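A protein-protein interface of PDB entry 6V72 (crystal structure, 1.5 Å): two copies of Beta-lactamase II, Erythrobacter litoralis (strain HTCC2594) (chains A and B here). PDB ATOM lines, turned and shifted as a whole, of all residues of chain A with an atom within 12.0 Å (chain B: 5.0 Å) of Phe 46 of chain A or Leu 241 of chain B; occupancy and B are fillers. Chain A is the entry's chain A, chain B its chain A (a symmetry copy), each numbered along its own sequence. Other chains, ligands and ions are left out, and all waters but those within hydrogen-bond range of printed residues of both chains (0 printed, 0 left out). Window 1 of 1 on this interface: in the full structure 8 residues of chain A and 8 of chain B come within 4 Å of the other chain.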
ATOM      1  N   SER A   9     -17.349 -33.476  17.911  1.00  0.00           N
ATOM      2  CA  SER A   9     -16.418 -34.589  18.091  1.00  0.00           C
ATOM      3  C   SER A   9     -15.060 -34.272  17.465  1.00  0.00           C
ATOM      4  O   SER A   9     -14.966 -33.461  16.539  1.00  0.00           O
ATOM      5  CB  SER A   9     -16.969 -35.876  17.472  1.00  0.00           C
ATOM      6  OG  SER A   9     -16.808 -35.883  16.061  1.00  0.00           O
ATOM      7  N   VAL A  10     -14.005 -34.924  17.960  1.00  0.00           N
ATOM      8  CA  VAL A  10     -12.684 -34.739  17.361  1.00  0.00           C
ATOM      9  C   VAL A  10     -12.684 -35.222  15.912  1.00  0.00           C
ATOM     10  O   VAL A  10     -12.125 -34.565  15.022  1.00  0.00           O
ATOM     11  CB  VAL A  10     -11.607 -35.455  18.195  1.00  0.00           C
ATOM     12  CG1 VAL A  10     -10.257 -35.399  17.480  1.00  0.00           C
ATOM     13  CG2 VAL A  10     -11.486 -34.813  19.572  1.00  0.00           C
ATOM     14  N   GLU A  12     -15.179 -35.365  13.737  1.00  0.00           N
ATOM     15  CA  GLU A  12     -15.852 -34.382  12.893  1.00  0.00           C
ATOM     16  C   GLU A  12     -14.988 -33.138  12.700  1.00  0.00           C
ATOM     17  O   GLU A  12     -14.960 -32.556  11.609  1.00  0.00           O
ATOM     18  CB  GLU A  12     -17.208 -34.015  13.497  1.00  0.00           C
ATOM     19  CG  GLU A  12     -18.245 -35.142  13.417  1.00  0.00           C
ATOM     20  CD  GLU A  12     -19.433 -34.930  14.346  1.00  0.00           C
ATOM     21  OE1 GLU A  12     -20.493 -35.554  14.120  1.00  0.00           O
ATOM     22  OE2 GLU A  12     -19.309 -34.143  15.309  1.00  0.00           O
ATOM     23  N   GLN A  13     -14.262 -32.727  13.745  1.00  0.00           N
ATOM     24  CA  GLN A  13     -13.464 -31.509  13.648  1.00  0.00           C
ATOM     25  C   GLN A  13     -12.256 -31.697  12.743  1.00  0.00           C
ATOM     26  O   GLN A  13     -11.769 -30.724  12.158  1.00  0.00           O
ATOM     27  CB  GLN A  13     -13.008 -31.051  15.035  1.00  0.00           C
ATOM     28  CG  GLN A  13     -14.115 -30.526  15.936  1.00  0.00           C
ATOM     29  CD  GLN A  13     -13.576 -30.028  17.266  1.00  0.00           C
ATOM     30  OE1 GLN A  13     -12.662 -29.200  17.305  1.00  0.00           O
ATOM     31  NE2 GLN A  13     -14.119 -30.555  18.366  1.00  0.00           N
ATOM     32  N   TYR A  40      -7.104 -31.381  22.745  1.00  0.00           N
ATOM     33  CA  TYR A  40      -8.506 -31.169  23.070  1.00  0.00           C
ATOM     34  C   TYR A  40      -8.728 -31.256  24.567  1.00  0.00           C
ATOM     35  O   TYR A  40      -8.059 -32.008  25.289  1.00  0.00           O
ATOM     36  CB  TYR A  40      -9.430 -32.183  22.361  1.00  0.00           C
ATOM     37  CG  TYR A  40      -9.355 -32.060  20.865  1.00  0.00           C
ATOM     38  CD1 TYR A  40      -8.389 -32.751  20.136  1.00  0.00           C
ATOM     39  CD2 TYR A  40     -10.216 -31.214  20.173  1.00  0.00           C
ATOM     40  CE1 TYR A  40      -8.303 -32.622  18.765  1.00  0.00           C
ATOM     41  CE2 TYR A  40     -10.140 -31.080  18.798  1.00  0.00           C
ATOM     42  CZ  TYR A  40      -9.181 -31.785  18.099  1.00  0.00           C
ATOM     43  OH  TYR A  40      -9.089 -31.661  16.728  1.00  0.00           O
ATOM     44  N   LEU A  41      -9.693 -30.476  25.020  1.00  0.00           N
ATOM     45  CA  LEU A  41     -10.097 -30.504  26.408  1.00  0.00           C
ATOM     46  C   LEU A  41     -11.607 -30.623  26.449  1.00  0.00           C
ATOM     47  O   LEU A  41     -12.307 -29.908  25.728  1.00  0.00           O
ATOM     48  CB  LEU A  41      -9.619 -29.242  27.118  1.00  0.00           C
ATOM     49  CG  LEU A  41     -10.026 -29.179  28.573  1.00  0.00           C
ATOM     50  CD1 LEU A  41      -9.050 -30.045  29.343  1.00  0.00           C
ATOM     51  CD2 LEU A  41      -9.932 -27.754  29.038  1.00  0.00           C
ATOM     52  N   ASP A  42     -12.102 -31.531  27.281  1.00  0.00           N
ATOM     53  CA  ASP A  42     -13.530 -31.697  27.524  1.00  0.00           C
ATOM     54  C   ASP A  42     -13.729 -31.805  29.039  1.00  0.00           C
ATOM     55  O   ASP A  42     -14.060 -32.872  29.557  1.00  0.00           O
ATOM     56  CB  ASP A  42     -14.067 -32.926  26.796  1.00  0.00           C
ATOM     57  CG  ASP A  42     -15.575 -32.961  26.755  1.00  0.00           C
ATOM     58  OD1 ASP A  42     -16.130 -33.836  26.054  1.00  0.00           O
ATOM     59  OD2 ASP A  42     -16.204 -32.103  27.406  1.00  0.00           O
ATOM     60  N   LEU A  43     -13.517 -30.690  29.751  1.00  0.00           N
ATOM     61  CA  LEU A  43     -13.444 -30.759  31.212  1.00  0.00           C
ATOM     62  C   LEU A  43     -14.815 -30.983  31.845  1.00  0.00           C
ATOM     63  O   LEU A  43     -14.947 -31.786  32.776  1.00  0.00           O
ATOM     64  CB  LEU A  43     -12.799 -29.492  31.782  1.00  0.00           C
ATOM     65  CG  LEU A  43     -11.279 -29.542  31.959  1.00  0.00           C
ATOM     66  CD1 LEU A  43     -10.764 -28.406  32.838  1.00  0.00           C
ATOM     67  CD2 LEU A  43     -10.826 -30.905  32.487  1.00  0.00           C
ATOM     68  N   MET A  44     -15.841 -30.280  31.379  1.00  0.00           N
ATOM     69  CA  MET A  44     -17.147 -30.399  32.018  1.00  0.00           C
ATOM     70  C   MET A  44     -18.083 -31.328  31.253  1.00  0.00           C
ATOM     71  O   MET A  44     -19.261 -31.449  31.586  1.00  0.00           O
ATOM     72  CB  MET A  44     -17.780 -29.016  32.193  1.00  0.00           C
ATOM     73  CG  MET A  44     -16.890 -28.045  32.949  1.00  0.00           C
ATOM     74  SD  MET A  44     -17.119 -28.219  34.894  1.00  0.00           S
ATOM     75  CE  MET A  44     -19.051 -28.340  35.003  1.00  0.00           C
ATOM     76  N   GLY A  45     -17.545 -32.000  30.242  1.00  0.00           N
ATOM     77  CA  GLY A  45     -18.318 -32.940  29.461  1.00  0.00           C
ATOM     78  C   GLY A  45     -19.122 -32.339  28.333  1.00  0.00           C
ATOM     79  O   GLY A  45     -19.935 -33.051  27.732  1.00  0.00           O
ATOM     80  N   PHE A  46     -18.916 -31.060  28.012  1.00  0.00           N
ATOM     81  CA  PHE A  46     -19.741 -30.380  27.019  1.00  0.00           C
ATOM     82  C   PHE A  46     -19.271 -30.608  25.586  1.00  0.00           C
ATOM     83  O   PHE A  46     -19.976 -30.211  24.652  1.00  0.00           O
ATOM     84  CB  PHE A  46     -19.773 -28.874  27.300  1.00  0.00           C
ATOM     85  CG  PHE A  46     -20.189 -28.518  28.701  1.00  0.00           C
ATOM     86  CD1 PHE A  46     -20.997 -29.361  29.445  1.00  0.00           C
ATOM     87  CD2 PHE A  46     -19.781 -27.323  29.269  1.00  0.00           C
ATOM     88  CE1 PHE A  46     -21.384 -29.022  30.739  1.00  0.00           C
ATOM     89  CE2 PHE A  46     -20.166 -26.977  30.559  1.00  0.00           C
ATOM     90  CZ  PHE A  46     -20.970 -27.827  31.294  1.00  0.00           C
ATOM     91  N   GLY A  47     -18.111 -31.224  25.388  1.00  0.00           N
ATOM     92  CA  GLY A  47     -17.588 -31.458  24.064  1.00  0.00           C
ATOM     93  C   GLY A  47     -16.141 -31.024  23.979  1.00  0.00           C
ATOM     94  O   GLY A  47     -15.714 -30.100  24.675  1.00  0.00           O
ATOM     95  N   PRO A  48     -15.353 -31.684  23.130  1.00  0.00           N
ATOM     96  CA  PRO A  48     -13.915 -31.367  23.066  1.00  0.00           C
ATOM     97  C   PRO A  48     -13.663 -30.042  22.357  1.00  0.00           C
ATOM     98  O   PRO A  48     -14.149 -29.817  21.248  1.00  0.00           O
ATOM     99  CB  PRO A  48     -13.326 -32.546  22.277  1.00  0.00           C
ATOM    100  CG  PRO A  48     -14.474 -33.033  21.424  1.00  0.00           C
ATOM    101  CD  PRO A  48     -15.720 -32.814  22.254  1.00  0.00           C
ATOM    102  N   ILE A  49     -12.885 -29.180  22.999  1.00  0.00           N
ATOM    103  CA  ILE A  49     -12.515 -27.866  22.475  1.00  0.00           C
ATOM    104  C   ILE A  49     -11.052 -27.921  22.060  1.00  0.00           C
ATOM    105  O   ILE A  49     -10.212 -28.358  22.855  1.00  0.00           O
ATOM    106  CB  ILE A  49     -12.733 -26.750  23.515  1.00  0.00           C
ATOM    107  CG1 ILE A  49     -14.193 -26.717  23.977  1.00  0.00           C
ATOM    108  CG2 ILE A  49     -12.299 -25.389  22.954  1.00  0.00           C
ATOM    109  CD1 ILE A  49     -14.587 -25.410  24.630  1.00  0.00           C
ATOM    110  N   PRO A  50     -10.704 -27.492  20.851  1.00  0.00           N
ATOM    111  CA  PRO A  50      -9.302 -27.545  20.436  1.00  0.00           C
ATOM    112  C   PRO A  50      -8.485 -26.387  20.982  1.00  0.00           C
ATOM    113  O   PRO A  50      -8.982 -25.279  21.187  1.00  0.00           O
ATOM    114  CB  PRO A  50      -9.389 -27.453  18.905  1.00  0.00           C
ATOM    115  CG  PRO A  50     -10.639 -26.586  18.690  1.00  0.00           C
ATOM    116  CD  PRO A  50     -11.598 -27.006  19.776  1.00  0.00           C
ATOM    117  N   TRP A  69      -3.041 -28.132  26.108  1.00  0.00           N
ATOM    118  CA  TRP A  69      -3.897 -27.902  27.266  1.00  0.00           C
ATOM    119  C   TRP A  69      -3.240 -28.384  28.552  1.00  0.00           C
ATOM    120  O   TRP A  69      -3.415 -27.774  29.612  1.00  0.00           O
ATOM    121  CB  TRP A  69      -5.233 -28.616  27.107  1.00  0.00           C
ATOM    122  CG  TRP A  69      -6.239 -28.010  26.163  1.00  0.00           C
ATOM    123  CD1 TRP A  69      -6.648 -28.530  24.971  1.00  0.00           C
ATOM    124  CD2 TRP A  69      -7.031 -26.830  26.373  1.00  0.00           C
ATOM    125  NE1 TRP A  69      -7.621 -27.744  24.413  1.00  0.00           N
ATOM    126  CE2 TRP A  69      -7.878 -26.693  25.249  1.00  0.00           C
ATOM    127  CE3 TRP A  69      -7.099 -25.875  27.388  1.00  0.00           C
ATOM    128  CZ2 TRP A  69      -8.773 -25.636  25.113  1.00  0.00           C
ATOM    129  CZ3 TRP A  69      -8.000 -24.831  27.253  1.00  0.00           C
ATOM    130  CH2 TRP A  69      -8.812 -24.720  26.123  1.00  0.00           C
ATOM    131  N   GLY A 195     -15.872 -14.755  22.242  1.00  0.00           N
ATOM    132  CA  GLY A 195     -15.646 -15.649  23.344  1.00  0.00           C
ATOM    133  C   GLY A 195     -15.639 -14.896  24.646  1.00  0.00           C
ATOM    134  O   GLY A 195     -16.404 -13.943  24.865  1.00  0.00           O
ATOM    135  N   ASN A 196     -14.747 -15.342  25.524  1.00  0.00           N
ATOM    136  CA  ASN A 196     -14.633 -14.832  26.878  1.00  0.00           C
ATOM    137  C   ASN A 196     -13.803 -13.552  26.882  1.00  0.00           C
ATOM    138  O   ASN A 196     -12.582 -13.585  26.631  1.00  0.00           O
ATOM    139  CB  ASN A 196     -14.014 -15.900  27.772  1.00  0.00           C
ATOM    140  CG  ASN A 196     -14.100 -15.537  29.212  1.00  0.00           C
ATOM    141  OD1 ASN A 196     -14.013 -14.373  29.543  1.00  0.00           O
ATOM    142  ND2 ASN A 196     -14.292 -16.527  30.088  1.00  0.00           N
ATOM    143  N   ALA A 198     -13.622 -11.666  29.676  1.00  0.00           N
ATOM    144  CA  ALA A 198     -13.487 -11.310  31.086  1.00  0.00           C
ATOM    145  C   ALA A 198     -12.178 -10.587  31.376  1.00  0.00           C
ATOM    146  O   ALA A 198     -12.140  -9.734  32.266  1.00  0.00           O
ATOM    147  CB  ALA A 198     -13.610 -12.558  31.964  1.00  0.00           C
ATOM    148  N   ALA B 191     -26.211 -24.708  27.940  1.00  0.00           N
ATOM    149  CA  ALA B 191     -25.202 -23.728  27.587  1.00  0.00           C
ATOM    150  C   ALA B 191     -23.800 -24.245  27.883  1.00  0.00           C
ATOM    151  O   ALA B 191     -23.568 -25.012  28.832  1.00  0.00           O
ATOM    152  CB  ALA B 191     -25.438 -22.433  28.357  1.00  0.00           C
ATOM    153  N   SER B 192     -22.849 -23.798  27.078  1.00  0.00           N
ATOM    154  CA  SER B 192     -21.451 -24.136  27.306  1.00  0.00           C
ATOM    155  C   SER B 192     -20.617 -22.934  27.702  1.00  0.00           C
ATOM    156  O   SER B 192     -19.420 -23.089  27.944  1.00  0.00           O
ATOM    157  CB  SER B 192     -20.843 -24.803  26.065  1.00  0.00           C
ATOM    158  OG  SER B 192     -20.998 -23.988  24.915  1.00  0.00           O
ATOM    159  N   ASN B 193     -21.214 -21.749  27.797  1.00  0.00           N
ATOM    160  CA  ASN B 193     -20.486 -20.588  28.282  1.00  0.00           C
ATOM    161  C   ASN B 193     -21.505 -19.571  28.777  1.00  0.00           C
ATOM    162  O   ASN B 193     -22.714 -19.738  28.588  1.00  0.00           O
ATOM    163  CB  ASN B 193     -19.568 -20.014  27.194  1.00  0.00           C
ATOM    164  CG  ASN B 193     -20.329 -19.474  26.022  1.00  0.00           C
ATOM    165  OD1 ASN B 193     -21.050 -18.486  26.147  1.00  0.00           O
ATOM    166  ND2 ASN B 193     -20.164 -20.105  24.858  1.00  0.00           N
ATOM    167  N   LEU B 194     -21.002 -18.517  29.431  1.00  0.00           N
ATOM    168  CA  LEU B 194     -21.837 -17.476  30.015  1.00  0.00           C
ATOM    169  C   LEU B 194     -21.930 -16.253  29.122  1.00  0.00           C
ATOM    170  O   LEU B 194     -22.317 -15.175  29.590  1.00  0.00           O
ATOM    171  CB  LEU B 194     -21.314 -17.078  31.396  1.00  0.00           C
ATOM    172  CG  LEU B 194     -21.441 -18.178  32.448  1.00  0.00           C
ATOM    173  CD1 LEU B 194     -20.679 -17.801  33.709  1.00  0.00           C
ATOM    174  CD2 LEU B 194     -22.910 -18.455  32.748  1.00  0.00           C
ATOM    175  N   ARG B 237     -26.856 -25.421  35.335  1.00  0.00           N
ATOM    176  CA  ARG B 237     -25.787 -25.232  34.371  1.00  0.00           C
ATOM    177  C   ARG B 237     -25.135 -23.874  34.540  1.00  0.00           C
ATOM    178  O   ARG B 237     -23.910 -23.773  34.486  1.00  0.00           O
ATOM    179  CB  ARG B 237     -26.303 -25.406  32.941  1.00  0.00           C
ATOM    180  CG  ARG B 237     -25.273 -25.116  31.861  1.00  0.00           C
ATOM    181  CD  ARG B 237     -24.051 -26.033  31.928  1.00  0.00           C
ATOM    182  NE  ARG B 237     -24.383 -27.455  31.938  1.00  0.00           N
ATOM    183  CZ  ARG B 237     -24.561 -28.194  30.839  1.00  0.00           C
ATOM    184  NH1 ARG B 237     -24.856 -29.494  30.942  1.00  0.00           N
ATOM    185  NH2 ARG B 237     -24.455 -27.635  29.632  1.00  0.00           N
ATOM    186  N   THR B 238     -25.935 -22.810  34.708  1.00  0.00           N
ATOM    187  CA  THR B 238     -25.343 -21.493  34.904  1.00  0.00           C
ATOM    188  C   THR B 238     -24.407 -21.485  36.110  1.00  0.00           C
ATOM    189  O   THR B 238     -23.303 -20.937  36.040  1.00  0.00           O
ATOM    190  CB  THR B 238     -26.434 -20.428  35.066  1.00  0.00           C
ATOM    191  OG1 THR B 238     -27.264 -20.448  33.890  1.00  0.00           O
ATOM    192  CG2 THR B 238     -25.784 -19.031  35.258  1.00  0.00           C
ATOM    193  N   LEU B 239     -24.838 -22.100  37.214  1.00  0.00           N
ATOM    194  CA  LEU B 239     -24.009 -22.189  38.411  1.00  0.00           C
ATOM    195  C   LEU B 239     -22.714 -22.943  38.126  1.00  0.00           C
ATOM    196  O   LEU B 239     -21.622 -22.507  38.517  1.00  0.00           O
ATOM    197  CB  LEU B 239     -24.798 -22.898  39.520  1.00  0.00           C
ATOM    198  CG  LEU B 239     -24.078 -23.025  40.854  1.00  0.00           C
ATOM    199  CD1 LEU B 239     -23.504 -21.665  41.319  1.00  0.00           C
ATOM    200  CD2 LEU B 239     -25.035 -23.596  41.872  1.00  0.00           C
ATOM    201  N   ASP B 240     -22.818 -24.084  37.442  1.00  0.00           N
ATOM    202  CA  ASP B 240     -21.609 -24.843  37.122  1.00  0.00           C
ATOM    203  C   ASP B 240     -20.639 -23.996  36.301  1.00  0.00           C
ATOM    204  O   ASP B 240     -19.423 -23.999  36.552  1.00  0.00           O
ATOM    205  CB  ASP B 240     -21.965 -26.109  36.346  1.00  0.00           C
ATOM    206  CG  ASP B 240     -22.098 -27.357  37.233  1.00  0.00           C
ATOM    207  OD1 ASP B 240     -21.475 -27.423  38.326  1.00  0.00           O
ATOM    208  OD2 ASP B 240     -22.810 -28.291  36.806  1.00  0.00           O
ATOM    209  N   LEU B 241     -21.149 -23.281  35.296  1.00  0.00           N
ATOM    210  CA  LEU B 241     -20.269 -22.440  34.489  1.00  0.00           C
ATOM    211  C   LEU B 241     -19.650 -21.333  35.331  1.00  0.00           C
ATOM    212  O   LEU B 241     -18.461 -21.017  35.187  1.00  0.00           O
ATOM    213  CB  LEU B 241     -21.040 -21.833  33.315  1.00  0.00           C
ATOM    214  CG  LEU B 241     -21.502 -22.821  32.254  1.00  0.00           C
ATOM    215  CD1 LEU B 241     -22.464 -22.126  31.289  1.00  0.00           C
ATOM    216  CD2 LEU B 241     -20.282 -23.394  31.510  1.00  0.00           C
ATOM    217  N   ALA B 242     -20.455 -20.717  36.204  1.00  0.00           N
ATOM    218  CA  ALA B 242     -19.958 -19.621  37.030  1.00  0.00           C
ATOM    219  C   ALA B 242     -18.902 -20.098  38.020  1.00  0.00           C
ATOM    220  O   ALA B 242     -17.983 -19.334  38.359  1.00  0.00           O
ATOM    221  CB  ALA B 242     -21.129 -18.956  37.765  1.00  0.00           C
ATOM    222  N   GLU B 243     -19.005 -21.350  38.484  1.00  0.00           N
ATOM    223  CA  GLU B 243     -18.009 -21.878  39.415  1.00  0.00           C
ATOM    224  C   GLU B 243     -16.647 -22.069  38.767  1.00  0.00           C
ATOM    225  O   GLU B 243     -15.648 -22.185  39.488  1.00  0.00           O
ATOM    226  CB  GLU B 243     -18.485 -23.206  40.003  1.00  0.00           C
ATOM    227  CG  GLU B 243     -19.618 -23.035  41.004  1.00  0.00           C
ATOM    228  CD  GLU B 243     -20.349 -24.344  41.362  1.00  0.00           C
ATOM    229  OE1 GLU B 243     -20.323 -25.328  40.564  1.00  0.00           O
ATOM    230  OE2 GLU B 243     -20.968 -24.378  42.452  1.00  0.00           O
ATOM    231  N   GLU B 244     -16.575 -22.079  37.438  1.00  0.00           N
ATOM    232  CA  GLU B 244     -15.306 -22.239  36.730  1.00  0.00           C
ATOM    233  C   GLU B 244     -14.626 -20.918  36.394  1.00  0.00           C
ATOM    234  O   GLU B 244     -13.528 -20.934  35.814  1.00  0.00           O
ATOM    235  CB  GLU B 244     -15.510 -23.046  35.445  1.00  0.00           C
ATOM    236  CG  GLU B 244     -16.068 -24.451  35.675  1.00  0.00           C
ATOM    237  CD  GLU B 244     -15.226 -25.287  36.645  1.00  0.00           C
ATOM    238  OE1 GLU B 244     -13.983 -25.332  36.498  1.00  0.00           O
ATOM    239  OE2 GLU B 244     -15.816 -25.914  37.554  1.00  0.00           O
ATOM    240  N   LEU B 245     -15.213 -19.787  36.777  1.00  0.00           N
ATOM    241  CA  LEU B 245     -14.661 -18.479  36.404  1.00  0.00           C
ATOM    242  C   LEU B 245     -13.425 -18.131  37.236  1.00  0.00           C
ATOM    243  O   LEU B 245     -13.277 -18.610  38.360  1.00  0.00           O
ATOM    244  CB  LEU B 245     -15.713 -17.382  36.562  1.00  0.00           C
ATOM    245  CG  LEU B 245     -16.880 -17.474  35.582  1.00  0.00           C
ATOM    246  CD1 LEU B 245     -17.902 -16.374  35.870  1.00  0.00           C
ATOM    247  CD2 LEU B 245     -16.362 -17.362  34.151  1.00  0.00           C
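Met 44 of chain A touches Asp 240 of chain B. Phe 46 of chain A touches Arg 237 of chain B. Phe 46 of chain A touches Leu 241 of chain B.
No position is printed for both chains.
Printed residues of chain B within 4 Å of Met 44 of chain A: Asp 240 (3.9 Å) and Glu 244 (3.8 Å). Phe 46 of chain A touches two residues of chain B. Gly 195 of chain A touches none of the printed residues of chain B. Ser 192 of chain B touches none of the printed residues of chain A. No residue of chain A comes within 4 Å of Leu 194 of chain B. Printed residues of chain A within 4 Å of Arg 237 of chain B: Phe 46. No residue of chain A comes within 4 Å of Leu 239 of chain B. Asp 240 of chain B touches just one residue of chain A: Met 44. Of chain A, only Phe 46 (3.7 Å) comes within 4 Å of Leu 241 of chain B. Ala 242 of chain B touches none of the printed residues of chain A. No residue of chain A comes within 4 Å of Glu 243 of chain B. Of chain A, only Met 44 comes within 4 Å of Glu 244 of chain B. The nearest residue of chain B that does not touch Phe 46 of chain A is Ser 192 of chain B (4.1 Å).
The side-chain carboxylate of Glu 244 of chain B sits close to the side-chain sulfur of Met 44 of chain A (3.8 Å).
The side-chain carboxylate (OD2) of Asp 42 of chain A is in hydrogen-bond range of the backbone NH (N) of Phe 46 of chain A (3.0 Å). O of Ala 191 of chain B sits at hydrogen-bond distance from NH2 of Arg 237 of chain B (2.9 Å).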
